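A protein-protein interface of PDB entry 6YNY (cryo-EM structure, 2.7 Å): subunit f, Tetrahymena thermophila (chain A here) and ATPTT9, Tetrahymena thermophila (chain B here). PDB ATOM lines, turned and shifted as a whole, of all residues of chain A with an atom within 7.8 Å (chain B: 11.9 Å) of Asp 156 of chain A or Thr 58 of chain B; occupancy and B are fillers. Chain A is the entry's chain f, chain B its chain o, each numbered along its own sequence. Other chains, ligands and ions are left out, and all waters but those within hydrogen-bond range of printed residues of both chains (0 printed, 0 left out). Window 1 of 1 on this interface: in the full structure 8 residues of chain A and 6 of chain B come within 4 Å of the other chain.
The backbone NH (N) of Asn 57 of chain B is in hydrogen-bond range of a ring nitrogen (ND1) of His 155 of chain A, at 3.1 Å.
O of Gln 56 of chain B sits at hydrogen-bond distance from OG1 of Thr 59 of chain B (2.8 Å).
The side-chain amide oxygen of Asn 57 of chain B lies close to the side-chain hydroxyl of Thr 58 of chain B.
The backbone carbonyl oxygen (O) of His 151 of chain A sits at hydrogen-bond distance from the side-chain amide nitrogen (NE2) of Gln 157 of chain A, at 3.0 Å.
Asn 57 of chain B touches His 151 of chain A.
O of Tyr 154 of chain A touches CG of Gln 56 of chain B, 3.5 Å away.
His 155 of chain A touches Met 55 of chain B (CE1 to O, 3.2 Å).
CA of Gln 56 of chain B touches ND1 of His 155 of chain A, at 3.7 Å.
Asp 156 of chain A touches Thr 58 of chain B.
Thr 58 of chain B touches one residue of chain A.
Of chain B, only Asn 57 comes within 4 Å of His 151 of chain A.
No residue of chain B comes within 4 Å of Gln 157 of chain A.
Printed residues of chain A within 4 Å of Asn 57 of chain B: His 151 and His 155.
Printed residues of chain A within 4 Å of Met 55 of chain B: His 155.
Printed residues of chain B within 4 Å of Tyr 154 of chain A: Gln 56 (3.5 Å).
Val 62 of chain B touches none of the printed residues of chain A.
The nearest residue of chain B that does not touch Asp 156 of chain A is Asn 57 of chain B (4.6 Å).
The nearest printed residue of chain A that does not touch Met 55 of chain B is Tyr 154 of chain A (5.0 Å).
Printed residues of chain A that touch a printed residue of chain B: His 151, Tyr 154, His 155 and Asp 156.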
ATOM      1  N   GLN A 149      19.773  10.785 -35.317  1.00  0.00           N
ATOM      2  CA  GLN A 149      18.963  11.675 -34.496  1.00  0.00           C
ATOM      3  C   GLN A 149      18.909  11.237 -33.039  1.00  0.00           C
ATOM      4  O   GLN A 149      18.065  11.733 -32.285  1.00  0.00           O
ATOM      5  CB  GLN A 149      17.547  11.775 -35.063  1.00  0.00           C
ATOM      6  CG  GLN A 149      16.983  10.468 -35.558  1.00  0.00           C
ATOM      7  CD  GLN A 149      15.599  10.618 -36.133  1.00  0.00           C
ATOM      8  OE1 GLN A 149      14.772  11.359 -35.607  1.00  0.00           O
ATOM      9  NE2 GLN A 149      15.340   9.920 -37.226  1.00  0.00           N
ATOM     10  N   VAL A 150      19.779  10.324 -32.627  1.00  0.00           N
ATOM     11  CA  VAL A 150      19.852   9.912 -31.218  1.00  0.00           C
ATOM     12  C   VAL A 150      20.830  10.874 -30.557  1.00  0.00           C
ATOM     13  O   VAL A 150      22.017  10.597 -30.372  1.00  0.00           O
ATOM     14  CB  VAL A 150      20.258   8.446 -31.070  1.00  0.00           C
ATOM     15  CG1 VAL A 150      20.262   8.042 -29.622  1.00  0.00           C
ATOM     16  CG2 VAL A 150      19.311   7.577 -31.849  1.00  0.00           C
ATOM     17  N   HIS A 151      20.308  12.032 -30.174  1.00  0.00           N
ATOM     18  CA  HIS A 151      21.140  13.117 -29.677  1.00  0.00           C
ATOM     19  C   HIS A 151      21.748  12.741 -28.334  1.00  0.00           C
ATOM     20  O   HIS A 151      21.029  12.539 -27.350  1.00  0.00           O
ATOM     21  CB  HIS A 151      20.316  14.392 -29.566  1.00  0.00           C
ATOM     22  CG  HIS A 151      19.610  14.763 -30.832  1.00  0.00           C
ATOM     23  ND1 HIS A 151      20.281  15.088 -31.989  1.00  0.00           N
ATOM     24  CD2 HIS A 151      18.292  14.862 -31.121  1.00  0.00           C
ATOM     25  CE1 HIS A 151      19.407  15.367 -32.938  1.00  0.00           C
ATOM     26  NE2 HIS A 151      18.193  15.238 -32.437  1.00  0.00           N
ATOM     27  N   GLY A 153      23.531  14.632 -26.432  1.00  0.00           N
ATOM     28  CA  GLY A 153      23.594  15.765 -25.532  1.00  0.00           C
ATOM     29  C   GLY A 153      22.235  16.253 -25.084  1.00  0.00           C
ATOM     30  O   GLY A 153      21.299  15.468 -24.896  1.00  0.00           O
ATOM     31  N   TYR A 154      22.128  17.569 -24.918  1.00  0.00           N
ATOM     32  CA  TYR A 154      20.945  18.196 -24.335  1.00  0.00           C
ATOM     33  C   TYR A 154      19.975  18.602 -25.442  1.00  0.00           C
ATOM     34  O   TYR A 154      19.793  19.774 -25.769  1.00  0.00           O
ATOM     35  CB  TYR A 154      21.349  19.390 -23.484  1.00  0.00           C
ATOM     36  CG  TYR A 154      22.429  19.088 -22.479  1.00  0.00           C
ATOM     37  CD1 TYR A 154      22.362  17.961 -21.679  1.00  0.00           C
ATOM     38  CD2 TYR A 154      23.522  19.925 -22.338  1.00  0.00           C
ATOM     39  CE1 TYR A 154      23.344  17.684 -20.767  1.00  0.00           C
ATOM     40  CE2 TYR A 154      24.508  19.653 -21.427  1.00  0.00           C
ATOM     41  CZ  TYR A 154      24.417  18.532 -20.644  1.00  0.00           C
ATOM     42  OH  TYR A 154      25.406  18.261 -19.733  1.00  0.00           O
ATOM     43  N   HIS A 155      19.336  17.588 -26.013  1.00  0.00           N
ATOM     44  CA  HIS A 155      18.363  17.782 -27.071  1.00  0.00           C
ATOM     45  C   HIS A 155      17.238  16.778 -26.901  1.00  0.00           C
ATOM     46  O   HIS A 155      17.425  15.698 -26.335  1.00  0.00           O
ATOM     47  CB  HIS A 155      18.981  17.615 -28.460  1.00  0.00           C
ATOM     48  CG  HIS A 155      20.060  18.599 -28.769  1.00  0.00           C
ATOM     49  ND1 HIS A 155      19.796  19.896 -29.146  1.00  0.00           N
ATOM     50  CD2 HIS A 155      21.406  18.474 -28.768  1.00  0.00           C
ATOM     51  CE1 HIS A 155      20.934  20.529 -29.360  1.00  0.00           C
ATOM     52  NE2 HIS A 155      21.927  19.688 -29.137  1.00  0.00           N
ATOM     53  N   ASP A 156      16.066  17.150 -27.394  1.00  0.00           N
ATOM     54  CA  ASP A 156      14.939  16.237 -27.432  1.00  0.00           C
ATOM     55  C   ASP A 156      15.109  15.240 -28.567  1.00  0.00           C
ATOM     56  O   ASP A 156      15.504  15.601 -29.678  1.00  0.00           O
ATOM     57  CB  ASP A 156      13.632  17.004 -27.614  1.00  0.00           C
ATOM     58  CG  ASP A 156      13.288  17.868 -26.422  1.00  0.00           C
ATOM     59  OD1 ASP A 156      13.457  17.401 -25.279  1.00  0.00           O
ATOM     60  OD2 ASP A 156      12.843  19.017 -26.628  1.00  0.00           O
ATOM     61  N   GLN A 157      14.815  13.981 -28.279  1.00  0.00           N
ATOM     62  CA  GLN A 157      14.802  12.928 -29.279  1.00  0.00           C
ATOM     63  C   GLN A 157      13.371  12.635 -29.693  1.00  0.00           C
ATOM     64  O   GLN A 157      12.418  12.889 -28.952  1.00  0.00           O
ATOM     65  CB  GLN A 157      15.456  11.653 -28.750  1.00  0.00           C
ATOM     66  CG  GLN A 157      16.921  11.774 -28.461  1.00  0.00           C
ATOM     67  CD  GLN A 157      17.519  10.474 -27.989  1.00  0.00           C
ATOM     68  OE1 GLN A 157      16.900   9.418 -28.091  1.00  0.00           O
ATOM     69  NE2 GLN A 157      18.726  10.543 -27.465  1.00  0.00           N
ATOM     70  N   LYS A 158      13.225  12.100 -30.902  1.00  0.00           N
ATOM     71  CA  LYS A 158      11.928  11.692 -31.429  1.00  0.00           C
ATOM     72  C   LYS A 158      12.085  10.284 -31.985  1.00  0.00           C
ATOM     73  O   LYS A 158      12.429  10.096 -33.153  1.00  0.00           O
ATOM     74  CB  LYS A 158      11.427  12.655 -32.482  1.00  0.00           C
ATOM     75  CG  LYS A 158       9.977  12.447 -32.828  1.00  0.00           C
ATOM     76  CD  LYS A 158       9.531  13.368 -33.935  1.00  0.00           C
ATOM     77  CE  LYS A 158       8.040  13.248 -34.172  1.00  0.00           C
ATOM     78  NZ  LYS A 158       7.268  13.643 -32.971  1.00  0.00           N
ATOM     79  N   TRP A 159      11.836   9.297 -31.135  1.00  0.00           N
ATOM     80  CA  TRP A 159      11.891   7.915 -31.564  1.00  0.00           C
ATOM     81  C   TRP A 159      10.790   7.640 -32.580  1.00  0.00           C
ATOM     82  O   TRP A 159       9.793   8.361 -32.669  1.00  0.00           O
ATOM     83  CB  TRP A 159      11.746   6.975 -30.370  1.00  0.00           C
ATOM     84  CG  TRP A 159      12.912   6.959 -29.444  1.00  0.00           C
ATOM     85  CD1 TRP A 159      13.903   7.886 -29.354  1.00  0.00           C
ATOM     86  CD2 TRP A 159      13.211   5.959 -28.468  1.00  0.00           C
ATOM     87  NE1 TRP A 159      14.800   7.528 -28.384  1.00  0.00           N
ATOM     88  CE2 TRP A 159      14.397   6.346 -27.825  1.00  0.00           C
ATOM     89  CE3 TRP A 159      12.591   4.772 -28.078  1.00  0.00           C
ATOM     90  CZ2 TRP A 159      14.972   5.594 -26.815  1.00  0.00           C
ATOM     91  CZ3 TRP A 159      13.165   4.028 -27.078  1.00  0.00           C
ATOM     92  CH2 TRP A 159      14.343   4.439 -26.457  1.00  0.00           C
ATOM     93  N   MET B  55      23.341  24.498 -27.543  1.00  0.00           N
ATOM     94  CA  MET B  55      22.016  25.006 -27.206  1.00  0.00           C
ATOM     95  C   MET B  55      20.929  24.157 -27.865  1.00  0.00           C
ATOM     96  O   MET B  55      21.112  23.661 -28.975  1.00  0.00           O
ATOM     97  CB  MET B  55      21.892  26.466 -27.631  1.00  0.00           C
ATOM     98  CG  MET B  55      20.601  27.119 -27.218  1.00  0.00           C
ATOM     99  SD  MET B  55      20.739  28.911 -27.127  1.00  0.00           S
ATOM    100  CE  MET B  55      19.212  29.306 -26.291  1.00  0.00           C
ATOM    101  N   GLN B  56      19.799  23.996 -27.177  1.00  0.00           N
ATOM    102  CA  GLN B  56      18.732  23.130 -27.662  1.00  0.00           C
ATOM    103  C   GLN B  56      18.351  23.485 -29.092  1.00  0.00           C
ATOM    104  O   GLN B  56      18.154  24.654 -29.426  1.00  0.00           O
ATOM    105  CB  GLN B  56      17.504  23.232 -26.759  1.00  0.00           C
ATOM    106  CG  GLN B  56      17.583  22.445 -25.475  1.00  0.00           C
ATOM    107  CD  GLN B  56      18.207  23.225 -24.342  1.00  0.00           C
ATOM    108  OE1 GLN B  56      19.095  24.050 -24.550  1.00  0.00           O
ATOM    109  NE2 GLN B  56      17.733  22.977 -23.131  1.00  0.00           N
ATOM    110  N   ASN B  57      18.238  22.455 -29.932  1.00  0.00           N
ATOM    111  CA  ASN B  57      17.941  22.678 -31.341  1.00  0.00           C
ATOM    112  C   ASN B  57      16.521  23.190 -31.534  1.00  0.00           C
ATOM    113  O   ASN B  57      16.270  24.028 -32.405  1.00  0.00           O
ATOM    114  CB  ASN B  57      18.161  21.386 -32.126  1.00  0.00           C
ATOM    115  CG  ASN B  57      17.428  20.206 -31.522  1.00  0.00           C
ATOM    116  OD1 ASN B  57      16.571  20.370 -30.656  1.00  0.00           O
ATOM    117  ND2 ASN B  57      17.764  19.007 -31.972  1.00  0.00           N
ATOM    118  N   THR B  58      15.580  22.692 -30.738  1.00  0.00           N
ATOM    119  CA  THR B  58      14.180  23.090 -30.853  1.00  0.00           C
ATOM    120  C   THR B  58      13.876  24.227 -29.878  1.00  0.00           C
ATOM    121  O   THR B  58      12.989  24.146 -29.031  1.00  0.00           O
ATOM    122  CB  THR B  58      13.268  21.895 -30.605  1.00  0.00           C
ATOM    123  OG1 THR B  58      13.561  21.329 -29.324  1.00  0.00           O
ATOM    124  CG2 THR B  58      13.446  20.845 -31.675  1.00  0.00           C
ATOM    125  N   THR B  59      14.637  25.305 -30.021  1.00  0.00           N
ATOM    126  CA  THR B  59      14.488  26.494 -29.197  1.00  0.00           C
ATOM    127  C   THR B  59      13.985  27.646 -30.049  1.00  0.00           C
ATOM    128  O   THR B  59      14.570  27.956 -31.092  1.00  0.00           O
ATOM    129  CB  THR B  59      15.808  26.880 -28.534  1.00  0.00           C
ATOM    130  OG1 THR B  59      16.251  25.814 -27.691  1.00  0.00           O
ATOM    131  CG2 THR B  59      15.635  28.127 -27.707  1.00  0.00           C
ATOM    132  N   ASN B  60      12.908  28.276 -29.598  1.00  0.00           N
ATOM    133  CA  ASN B  60      12.304  29.393 -30.301  1.00  0.00           C
ATOM    134  C   ASN B  60      11.964  30.480 -29.296  1.00  0.00           C
ATOM    135  O   ASN B  60      11.577  30.189 -28.163  1.00  0.00           O
ATOM    136  CB  ASN B  60      11.041  28.968 -31.057  1.00  0.00           C
ATOM    137  CG  ASN B  60      11.307  27.896 -32.083  1.00  0.00           C
ATOM    138  OD1 ASN B  60      10.609  26.886 -32.135  1.00  0.00           O
ATOM    139  ND2 ASN B  60      12.321  28.105 -32.908  1.00  0.00           N
ATOM    140  N   ILE B  61      12.118  31.730 -29.719  1.00  0.00           N
ATOM    141  CA  ILE B  61      11.752  32.889 -28.916  1.00  0.00           C
ATOM    142  C   ILE B  61      10.528  33.516 -29.562  1.00  0.00           C
ATOM    143  O   ILE B  61      10.577  33.935 -30.724  1.00  0.00           O
ATOM    144  CB  ILE B  61      12.899  33.907 -28.822  1.00  0.00           C
ATOM    145  CG1 ILE B  61      14.186  33.252 -28.322  1.00  0.00           C
ATOM    146  CG2 ILE B  61      12.515  35.028 -27.897  1.00  0.00           C
ATOM    147  CD1 ILE B  61      14.172  32.891 -26.885  1.00  0.00           C
ATOM    148  N   VAL B  62       9.432  33.576 -28.816  1.00  0.00           N
ATOM    149  CA  VAL B  62       8.173  34.123 -29.299  1.00  0.00           C
ATOM    150  C   VAL B  62       7.904  35.433 -28.577  1.00  0.00           C
ATOM    151  O   VAL B  62       8.196  35.567 -27.384  1.00  0.00           O
ATOM    152  CB  VAL B  62       7.008  33.137 -29.097  1.00  0.00           C
ATOM    153  CG1 VAL B  62       5.748  33.686 -29.712  1.00  0.00           C
ATOM    154  CG2 VAL B  62       7.341  31.796 -29.713  1.00  0.00           C
ATOM    155  N   MET B  68      -0.253  26.687 -24.218  1.00  0.00           N
ATOM    156  CA  MET B  68       0.011  25.321 -24.637  1.00  0.00           C
ATOM    157  C   MET B  68      -0.970  24.361 -23.982  1.00  0.00           C
ATOM    158  O   MET B  68      -1.394  24.557 -22.841  1.00  0.00           O
ATOM    159  CB  MET B  68       1.440  24.915 -24.284  1.00  0.00           C
ATOM    160  CG  MET B  68       2.500  25.506 -25.190  1.00  0.00           C
ATOM    161  SD  MET B  68       2.508  24.741 -26.818  1.00  0.00           S
ATOM    162  CE  MET B  68       4.013  25.426 -27.488  1.00  0.00           C
ATOM    163  N   ASP B  75       1.605  17.917 -27.777  1.00  0.00           N
ATOM    164  CA  ASP B  75       2.185  19.203 -27.400  1.00  0.00           C
ATOM    165  C   ASP B  75       1.873  20.197 -28.506  1.00  0.00           C
ATOM    166  O   ASP B  75       2.387  20.065 -29.620  1.00  0.00           O
ATOM    167  CB  ASP B  75       3.692  19.087 -27.187  1.00  0.00           C
ATOM    168  CG  ASP B  75       4.329  20.397 -26.790  1.00  0.00           C
ATOM    169  OD1 ASP B  75       3.593  21.312 -26.365  1.00  0.00           O
ATOM    170  OD2 ASP B  75       5.565  20.519 -26.915  1.00  0.00           O
ATOM    171  N   ILE B  77      -0.230  24.379 -29.377  1.00  0.00           N
ATOM    172  CA  ILE B  77      -0.805  25.643 -28.939  1.00  0.00           C
ATOM    173  C   ILE B  77      -2.308  25.557 -29.149  1.00  0.00           C
ATOM    174  O   ILE B  77      -2.785  25.523 -30.287  1.00  0.00           O
ATOM    175  CB  ILE B  77      -0.200  26.828 -29.700  1.00  0.00           C
ATOM    176  CG1 ILE B  77       1.289  26.947 -29.383  1.00  0.00           C
ATOM    177  CG2 ILE B  77      -0.924  28.104 -29.349  1.00  0.00           C
ATOM    178  CD1 ILE B  77       2.039  27.849 -30.311  1.00  0.00           C
